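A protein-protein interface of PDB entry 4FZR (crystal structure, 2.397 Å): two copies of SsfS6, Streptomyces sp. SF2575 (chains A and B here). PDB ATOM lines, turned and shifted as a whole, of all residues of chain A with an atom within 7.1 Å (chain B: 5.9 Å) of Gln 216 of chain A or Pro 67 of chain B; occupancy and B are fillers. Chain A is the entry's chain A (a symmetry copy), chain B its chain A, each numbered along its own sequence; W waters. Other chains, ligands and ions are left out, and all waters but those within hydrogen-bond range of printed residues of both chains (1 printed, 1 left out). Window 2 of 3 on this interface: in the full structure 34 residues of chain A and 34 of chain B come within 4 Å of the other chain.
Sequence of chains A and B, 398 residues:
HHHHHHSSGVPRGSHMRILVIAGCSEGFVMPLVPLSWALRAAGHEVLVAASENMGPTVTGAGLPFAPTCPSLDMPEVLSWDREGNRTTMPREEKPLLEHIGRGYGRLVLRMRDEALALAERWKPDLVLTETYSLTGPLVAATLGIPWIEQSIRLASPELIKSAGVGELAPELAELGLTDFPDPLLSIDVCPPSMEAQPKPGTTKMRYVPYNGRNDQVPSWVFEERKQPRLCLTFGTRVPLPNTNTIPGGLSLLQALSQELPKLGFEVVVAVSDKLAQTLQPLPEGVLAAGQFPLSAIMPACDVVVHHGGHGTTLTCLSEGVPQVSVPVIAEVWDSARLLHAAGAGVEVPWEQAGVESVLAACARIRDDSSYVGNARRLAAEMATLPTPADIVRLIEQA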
ATOM      1  N   ASN A 214     -17.781  -6.572  -0.679  1.00  0.00           N
ATOM      2  CA  ASN A 214     -17.783  -6.612  -2.139  1.00  0.00           C
ATOM      3  C   ASN A 214     -18.741  -7.712  -2.595  1.00  0.00           C
ATOM      4  O   ASN A 214     -19.440  -8.299  -1.764  1.00  0.00           O
ATOM      5  CB  ASN A 214     -16.368  -6.813  -2.690  1.00  0.00           C
ATOM      6  CG  ASN A 214     -15.649  -5.496  -2.939  1.00  0.00           C
ATOM      7  OD1 ASN A 214     -15.253  -4.803  -2.001  1.00  0.00           O
ATOM      8  ND2 ASN A 214     -15.467  -5.151  -4.211  1.00  0.00           N
ATOM      9  N   ASP A 215     -18.804  -7.985  -3.896  1.00  0.00           N
ATOM     10  CA  ASP A 215     -19.876  -8.837  -4.400  1.00  0.00           C
ATOM     11  C   ASP A 215     -19.734  -9.280  -5.847  1.00  0.00           C
ATOM     12  O   ASP A 215     -19.211  -8.565  -6.694  1.00  0.00           O
ATOM     13  CB  ASP A 215     -21.185  -8.052  -4.315  1.00  0.00           C
ATOM     14  CG  ASP A 215     -22.390  -8.929  -4.063  1.00  0.00           C
ATOM     15  OD1 ASP A 215     -22.812  -9.644  -4.994  1.00  0.00           O
ATOM     16  OD2 ASP A 215     -22.928  -8.878  -2.938  1.00  0.00           O
ATOM     17  N   GLN A 216     -20.225 -10.483  -6.102  1.00  0.00           N
ATOM     18  CA  GLN A 216     -20.745 -10.875  -7.399  1.00  0.00           C
ATOM     19  C   GLN A 216     -21.421 -12.206  -7.155  1.00  0.00           C
ATOM     20  O   GLN A 216     -20.772 -13.247  -7.165  1.00  0.00           O
ATOM     21  CB  GLN A 216     -19.671 -11.017  -8.469  1.00  0.00           C
ATOM     22  CG  GLN A 216     -20.230 -11.687  -9.704  1.00  0.00           C
ATOM     23  CD  GLN A 216     -19.372 -11.504 -10.932  1.00  0.00           C
ATOM     24  OE1 GLN A 216     -18.615 -10.540 -11.048  1.00  0.00           O
ATOM     25  NE2 GLN A 216     -19.490 -12.439 -11.866  1.00  0.00           N
ATOM     26  N   VAL A 217     -22.720 -12.153  -6.876  1.00  0.00           N
ATOM     27  CA  VAL A 217     -23.489 -13.352  -6.570  1.00  0.00           C
ATOM     28  C   VAL A 217     -23.042 -14.458  -7.518  1.00  0.00           C
ATOM     29  O   VAL A 217     -23.489 -14.515  -8.668  1.00  0.00           O
ATOM     30  CB  VAL A 217     -25.005 -13.132  -6.740  1.00  0.00           C
ATOM     31  CG1 VAL A 217     -25.772 -14.337  -6.216  1.00  0.00           C
ATOM     32  CG2 VAL A 217     -25.461 -11.861  -6.022  1.00  0.00           C
ATOM     33  N   PRO A 218     -22.154 -15.343  -7.038  1.00  0.00           N
ATOM     34  CA  PRO A 218     -21.464 -16.279  -7.932  1.00  0.00           C
ATOM     35  C   PRO A 218     -22.418 -17.097  -8.793  1.00  0.00           C
ATOM     36  O   PRO A 218     -23.604 -17.208  -8.482  1.00  0.00           O
ATOM     37  CB  PRO A 218     -20.664 -17.175  -6.974  1.00  0.00           C
ATOM     38  CG  PRO A 218     -21.251 -16.955  -5.626  1.00  0.00           C
ATOM     39  CD  PRO A 218     -21.806 -15.568  -5.625  1.00  0.00           C
ATOM     40  N   SER A 219     -21.885 -17.654  -9.873  1.00  0.00           N
ATOM     41  CA  SER A 219     -22.681 -18.397 -10.839  1.00  0.00           C
ATOM     42  C   SER A 219     -23.635 -19.371 -10.157  1.00  0.00           C
ATOM     43  O   SER A 219     -24.849 -19.180 -10.170  1.00  0.00           O
ATOM     44  CB  SER A 219     -21.759 -19.165 -11.787  1.00  0.00           C
ATOM     45  OG  SER A 219     -22.490 -20.069 -12.596  1.00  0.00           O
ATOM     46  N   VAL A 221     -25.003 -19.931  -7.553  1.00  0.00           N
ATOM     47  CA  VAL A 221     -26.106 -19.501  -6.698  1.00  0.00           C
ATOM     48  C   VAL A 221     -27.411 -19.409  -7.484  1.00  0.00           C
ATOM     49  O   VAL A 221     -28.481 -19.734  -6.967  1.00  0.00           O
ATOM     50  CB  VAL A 221     -25.834 -18.135  -6.047  1.00  0.00           C
ATOM     51  CG1 VAL A 221     -26.988 -17.749  -5.130  1.00  0.00           C
ATOM     52  CG2 VAL A 221     -24.534 -18.172  -5.272  1.00  0.00           C
ATOM     53  N   PHE A 222     -27.316 -18.968  -8.734  1.00  0.00           N
ATOM     54  CA  PHE A 222     -28.494 -18.797  -9.574  1.00  0.00           C
ATOM     55  C   PHE A 222     -28.833 -20.073 -10.353  1.00  0.00           C
ATOM     56  O   PHE A 222     -29.943 -20.212 -10.866  1.00  0.00           O
ATOM     57  CB  PHE A 222     -28.293 -17.638 -10.552  1.00  0.00           C
ATOM     58  CG  PHE A 222     -28.069 -16.306  -9.889  1.00  0.00           C
ATOM     59  CD1 PHE A 222     -29.069 -15.720  -9.132  1.00  0.00           C
ATOM     60  CD2 PHE A 222     -26.867 -15.627 -10.045  1.00  0.00           C
ATOM     61  CE1 PHE A 222     -28.871 -14.490  -8.527  1.00  0.00           C
ATOM     62  CE2 PHE A 222     -26.666 -14.394  -9.442  1.00  0.00           C
ATOM     63  CZ  PHE A 222     -27.670 -13.825  -8.684  1.00  0.00           C
ATOM     64  N   GLN A 291     -14.665 -15.230   0.154  1.00  0.00           N
ATOM     65  CA  GLN A 291     -15.742 -14.492   0.799  1.00  0.00           C
ATOM     66  C   GLN A 291     -16.899 -14.287  -0.172  1.00  0.00           C
ATOM     67  O   GLN A 291     -16.713 -13.779  -1.279  1.00  0.00           O
ATOM     68  CB  GLN A 291     -15.239 -13.141   1.310  1.00  0.00           C
ATOM     69  CG  GLN A 291     -16.238 -12.403   2.192  1.00  0.00           C
ATOM     70  CD  GLN A 291     -16.599 -13.175   3.449  1.00  0.00           C
ATOM     71  OE1 GLN A 291     -17.644 -13.823   3.516  1.00  0.00           O
ATOM     72  NE2 GLN A 291     -15.734 -13.104   4.457  1.00  0.00           N
ATOM     73  N   PHE A 292     -18.094 -14.687   0.250  1.00  0.00           N
ATOM     74  CA  PHE A 292     -19.287 -14.543  -0.571  1.00  0.00           C
ATOM     75  C   PHE A 292     -20.332 -13.691   0.137  1.00  0.00           C
ATOM     76  O   PHE A 292     -20.350 -13.616   1.368  1.00  0.00           O
ATOM     77  CB  PHE A 292     -19.877 -15.917  -0.892  1.00  0.00           C
ATOM     78  CG  PHE A 292     -18.961 -16.792  -1.694  1.00  0.00           C
ATOM     79  CD1 PHE A 292     -18.708 -16.512  -3.026  1.00  0.00           C
ATOM     80  CD2 PHE A 292     -18.352 -17.893  -1.119  1.00  0.00           C
ATOM     81  CE1 PHE A 292     -17.863 -17.312  -3.769  1.00  0.00           C
ATOM     82  CE2 PHE A 292     -17.505 -18.698  -1.858  1.00  0.00           C
ATOM     83  CZ  PHE A 292     -17.263 -18.404  -3.185  1.00  0.00           C
ATOM     84  N   PRO A 293     -21.207 -13.036  -0.642  1.00  0.00           N
ATOM     85  CA  PRO A 293     -22.331 -12.333  -0.019  1.00  0.00           C
ATOM     86  C   PRO A 293     -23.204 -13.340   0.717  1.00  0.00           C
ATOM     87  O   PRO A 293     -24.062 -13.976   0.104  1.00  0.00           O
ATOM     88  CB  PRO A 293     -23.074 -11.725  -1.212  1.00  0.00           C
ATOM     89  CG  PRO A 293     -22.697 -12.587  -2.374  1.00  0.00           C
ATOM     90  CD  PRO A 293     -21.283 -13.006  -2.113  1.00  0.00           C
ATOM     91  N   VAL B  48     -28.909  -5.562  -8.027  1.00  0.00           N
ATOM     92  CA  VAL B  48     -28.570  -4.540  -9.011  1.00  0.00           C
ATOM     93  C   VAL B  48     -27.733  -5.150 -10.128  1.00  0.00           C
ATOM     94  O   VAL B  48     -26.649  -5.683  -9.886  1.00  0.00           O
ATOM     95  CB  VAL B  48     -27.805  -3.367  -8.378  1.00  0.00           C
ATOM     96  CG1 VAL B  48     -27.474  -2.316  -9.435  1.00  0.00           C
ATOM     97  CG2 VAL B  48     -28.621  -2.762  -7.248  1.00  0.00           C
ATOM     98  N   ALA B  49     -28.251  -5.078 -11.350  1.00  0.00           N
ATOM     99  CA  ALA B  49     -27.574  -5.651 -12.504  1.00  0.00           C
ATOM    100  C   ALA B  49     -27.038  -4.541 -13.406  1.00  0.00           C
ATOM    101  O   ALA B  49     -27.775  -3.635 -13.795  1.00  0.00           O
ATOM    102  CB  ALA B  49     -28.522  -6.562 -13.272  1.00  0.00           C
ATOM    103  N   ALA B  50     -25.748  -4.611 -13.727  1.00  0.00           N
ATOM    104  CA  ALA B  50     -25.103  -3.585 -14.541  1.00  0.00           C
ATOM    105  C   ALA B  50     -23.821  -4.127 -15.169  1.00  0.00           C
ATOM    106  O   ALA B  50     -23.472  -5.290 -14.971  1.00  0.00           O
ATOM    107  CB  ALA B  50     -24.804  -2.350 -13.696  1.00  0.00           C
ATOM    108  N   SER B  51     -23.126  -3.286 -15.930  1.00  0.00           N
ATOM    109  CA  SER B  51     -21.877  -3.690 -16.568  1.00  0.00           C
ATOM    110  C   SER B  51     -20.823  -4.054 -15.519  1.00  0.00           C
ATOM    111  O   SER B  51     -20.823  -3.516 -14.412  1.00  0.00           O
ATOM    112  CB  SER B  51     -21.357  -2.580 -17.484  1.00  0.00           C
ATOM    113  OG  SER B  51     -20.994  -1.429 -16.741  1.00  0.00           O
ATOM    114  N   GLU B  52     -19.928  -4.968 -15.881  1.00  0.00           N
ATOM    115  CA  GLU B  52     -18.915  -5.483 -14.965  1.00  0.00           C
ATOM    116  C   GLU B  52     -18.176  -4.373 -14.226  1.00  0.00           C
ATOM    117  O   GLU B  52     -17.845  -4.515 -13.046  1.00  0.00           O
ATOM    118  CB  GLU B  52     -17.903  -6.332 -15.735  1.00  0.00           C
ATOM    119  CG  GLU B  52     -16.803  -6.919 -14.866  1.00  0.00           C
ATOM    120  CD  GLU B  52     -17.275  -8.122 -14.074  1.00  0.00           C
ATOM    121  OE1 GLU B  52     -17.879  -9.030 -14.683  1.00  0.00           O
ATOM    122  OE2 GLU B  52     -17.051  -8.156 -12.844  1.00  0.00           O
ATOM    123  N   THR B  59     -21.474  -2.521  -5.075  1.00  0.00           N
ATOM    124  CA  THR B  59     -21.174  -3.163  -3.802  1.00  0.00           C
ATOM    125  C   THR B  59     -20.678  -2.136  -2.793  1.00  0.00           C
ATOM    126  O   THR B  59     -20.866  -2.294  -1.588  1.00  0.00           O
ATOM    127  CB  THR B  59     -20.138  -4.285  -3.964  1.00  0.00           C
ATOM    128  OG1 THR B  59     -18.852  -3.732  -4.271  1.00  0.00           O
ATOM    129  CG2 THR B  59     -20.568  -5.212  -5.070  1.00  0.00           C
ATOM    130  N   PHE B  65     -24.713  -7.300  -6.327  1.00  0.00           N
ATOM    131  CA  PHE B  65     -24.368  -7.001  -7.716  1.00  0.00           C
ATOM    132  C   PHE B  65     -24.286  -8.237  -8.610  1.00  0.00           C
ATOM    133  O   PHE B  65     -23.860  -9.302  -8.175  1.00  0.00           O
ATOM    134  CB  PHE B  65     -23.024  -6.272  -7.775  1.00  0.00           C
ATOM    135  CG  PHE B  65     -22.504  -6.080  -9.174  1.00  0.00           C
ATOM    136  CD1 PHE B  65     -23.030  -5.089  -9.990  1.00  0.00           C
ATOM    137  CD2 PHE B  65     -21.499  -6.892  -9.677  1.00  0.00           C
ATOM    138  CE1 PHE B  65     -22.559  -4.907 -11.278  1.00  0.00           C
ATOM    139  CE2 PHE B  65     -21.023  -6.713 -10.969  1.00  0.00           C
ATOM    140  CZ  PHE B  65     -21.555  -5.721 -11.769  1.00  0.00           C
ATOM    141  N   ALA B  66     -24.680  -8.069  -9.870  1.00  0.00           N
ATOM    142  CA  ALA B  66     -24.532  -9.109 -10.886  1.00  0.00           C
ATOM    143  C   ALA B  66     -24.249  -8.451 -12.236  1.00  0.00           C
ATOM    144  O   ALA B  66     -24.937  -7.507 -12.619  1.00  0.00           O
ATOM    145  CB  ALA B  66     -25.789  -9.961 -10.968  1.00  0.00           C
ATOM    146  N   PRO B  67     -23.237  -8.948 -12.966  1.00  0.00           N
ATOM    147  CA  PRO B  67     -22.821  -8.301 -14.216  1.00  0.00           C
ATOM    148  C   PRO B  67     -23.677  -8.711 -15.413  1.00  0.00           C
ATOM    149  O   PRO B  67     -24.030  -9.883 -15.534  1.00  0.00           O
ATOM    150  CB  PRO B  67     -21.388  -8.799 -14.391  1.00  0.00           C
ATOM    151  CG  PRO B  67     -21.403 -10.171 -13.779  1.00  0.00           C
ATOM    152  CD  PRO B  67     -22.410 -10.128 -12.653  1.00  0.00           C
ATOM    153  N   THR B  68     -24.006  -7.760 -16.283  1.00  0.00           N
ATOM    154  CA  THR B  68     -24.832  -8.046 -17.457  1.00  0.00           C
ATOM    155  C   THR B  68     -24.040  -7.940 -18.759  1.00  0.00           C
ATOM    156  O   THR B  68     -24.545  -8.276 -19.831  1.00  0.00           O
ATOM    157  CB  THR B  68     -26.052  -7.112 -17.525  1.00  0.00           C
ATOM    158  OG1 THR B  68     -25.620  -5.745 -17.530  1.00  0.00           O
ATOM    159  CG2 THR B  68     -26.965  -7.357 -16.333  1.00  0.00           C
ATOM    160  N   CYS B  69     -22.797  -7.482 -18.660  1.00  0.00           N
ATOM    161  CA  CYS B  69     -21.906  -7.419 -19.810  1.00  0.00           C
ATOM    162  C   CYS B  69     -20.512  -7.041 -19.322  1.00  0.00           C
ATOM    163  O   CYS B  69     -20.361  -6.537 -18.209  1.00  0.00           O
ATOM    164  CB  CYS B  69     -22.412  -6.409 -20.848  1.00  0.00           C
ATOM    165  SG  CYS B  69     -22.296  -4.667 -20.362  1.00  0.00           S
ATOM    166  N   GLU B 114     -27.522 -11.328 -21.053  1.00  0.00           N
ATOM    167  CA  GLU B 114     -27.175 -11.696 -19.686  1.00  0.00           C
ATOM    168  C   GLU B 114     -28.185 -11.160 -18.673  1.00  0.00           C
ATOM    169  O   GLU B 114     -28.348 -11.729 -17.595  1.00  0.00           O
ATOM    170  CB  GLU B 114     -25.768 -11.201 -19.339  1.00  0.00           C
ATOM    171  CG  GLU B 114     -24.657 -12.119 -19.816  1.00  0.00           C
ATOM    172  CD  GLU B 114     -24.811 -13.533 -19.287  1.00  0.00           C
ATOM    173  OE1 GLU B 114     -24.933 -13.697 -18.054  1.00  0.00           O
ATOM    174  OE2 GLU B 114     -24.817 -14.480 -20.104  1.00  0.00           O
ATOM    175  N   LEU B 118     -30.338 -13.746 -16.495  1.00  0.00           N
ATOM    176  CA  LEU B 118     -30.299 -13.536 -15.055  1.00  0.00           C
ATOM    177  C   LEU B 118     -31.710 -13.486 -14.472  1.00  0.00           C
ATOM    178  O   LEU B 118     -31.984 -14.102 -13.444  1.00  0.00           O
ATOM    179  CB  LEU B 118     -29.550 -12.241 -14.734  1.00  0.00           C
ATOM    180  CG  LEU B 118     -29.482 -11.848 -13.258  1.00  0.00           C
ATOM    181  CD1 LEU B 118     -28.750 -12.901 -12.430  1.00  0.00           C
ATOM    182  CD2 LEU B 118     -28.815 -10.491 -13.121  1.00  0.00           C
HETATM  183  O   HOH W   1     -17.440  -5.422  -6.888  1.00  0.00           O
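OD1 of Asp 215 of chain A sits at hydrogen-bond distance from N of Phe 65 of chain B (3.3 Å). The side-chain carboxylate of Glu 52 of chain B lies close to the side-chain amide oxygen of Gln 216 of chain A, at 3.4 Å. The backbone carbonyl oxygen (O) of Phe 65 of chain B sits at hydrogen-bond distance from the backbone NH (N) of Val 217 of chain A.
The backbone NH (N) of Val 217 of chain A sits at hydrogen-bond distance from the side-chain carboxylate (OD1) of Asp 215 of chain A (3.1 Å). The backbone NH of Glu 52 of chain B is in hydrogen-bond range of the backbone carbonyl oxygen of Cys 69 of chain B, at 2.8 Å.
No position is printed for both chains. Of the 8 pairs that touch across the chains among the printed residues, none has its exchanged pair printed and touching as well.
Among the printed residues, merely in contact across the chains: Asn 214 of chain A with Thr 59 of chain B (3.7 Å), Asp 215 of chain A with Thr 59 of chain B (3.0 Å), Gln 216 of chain A with Phe 65 of chain B (3.6 Å), Gln 216 of chain A with Pro 67 of chain B (3.5 Å) and Phe 222 of chain A with Leu 118 of chain B (3.9 Å).
Water W1 lies within hydrogen-bond range of ND2 of Asn 214 of chain A (3.3 Å) and OG1 of Thr 59 of chain B (3.4 Å).
Of the 13 printed residues of chain B, 5 touch a printed residue of chain A. Hydrophobic or aromatic side chains of chain A that line the printed part of chain B: Val 217 and Phe 222.
Printed residues of chain B within 4 Å of Asp 215 of chain A: Thr 59 and Phe 65. Gln 216 of chain A touches just these residues of chain B: Glu 52 (3.4 Å), Phe 65 (3.6 Å) and Pro 67 (3.5 Å). Printed residues of chain B within 4 Å of Phe 222 of chain A: Leu 118 (3.9 Å). Of the printed residues of chain A, Glu 52 of chain B touches Gln 216. Pro 67 of chain B touches just one residue of chain A: Gln 216 (3.5 Å). Thr 68 of chain B touches none of the printed residues of chain A. The nearest residue of chain A that does not touch Pro 67 of chain B is Val 217 of chain A (6.0 Å). The nearest printed residue of chain B that does not touch Val 217 of chain A is Ala 66 of chain B (5.3 Å).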
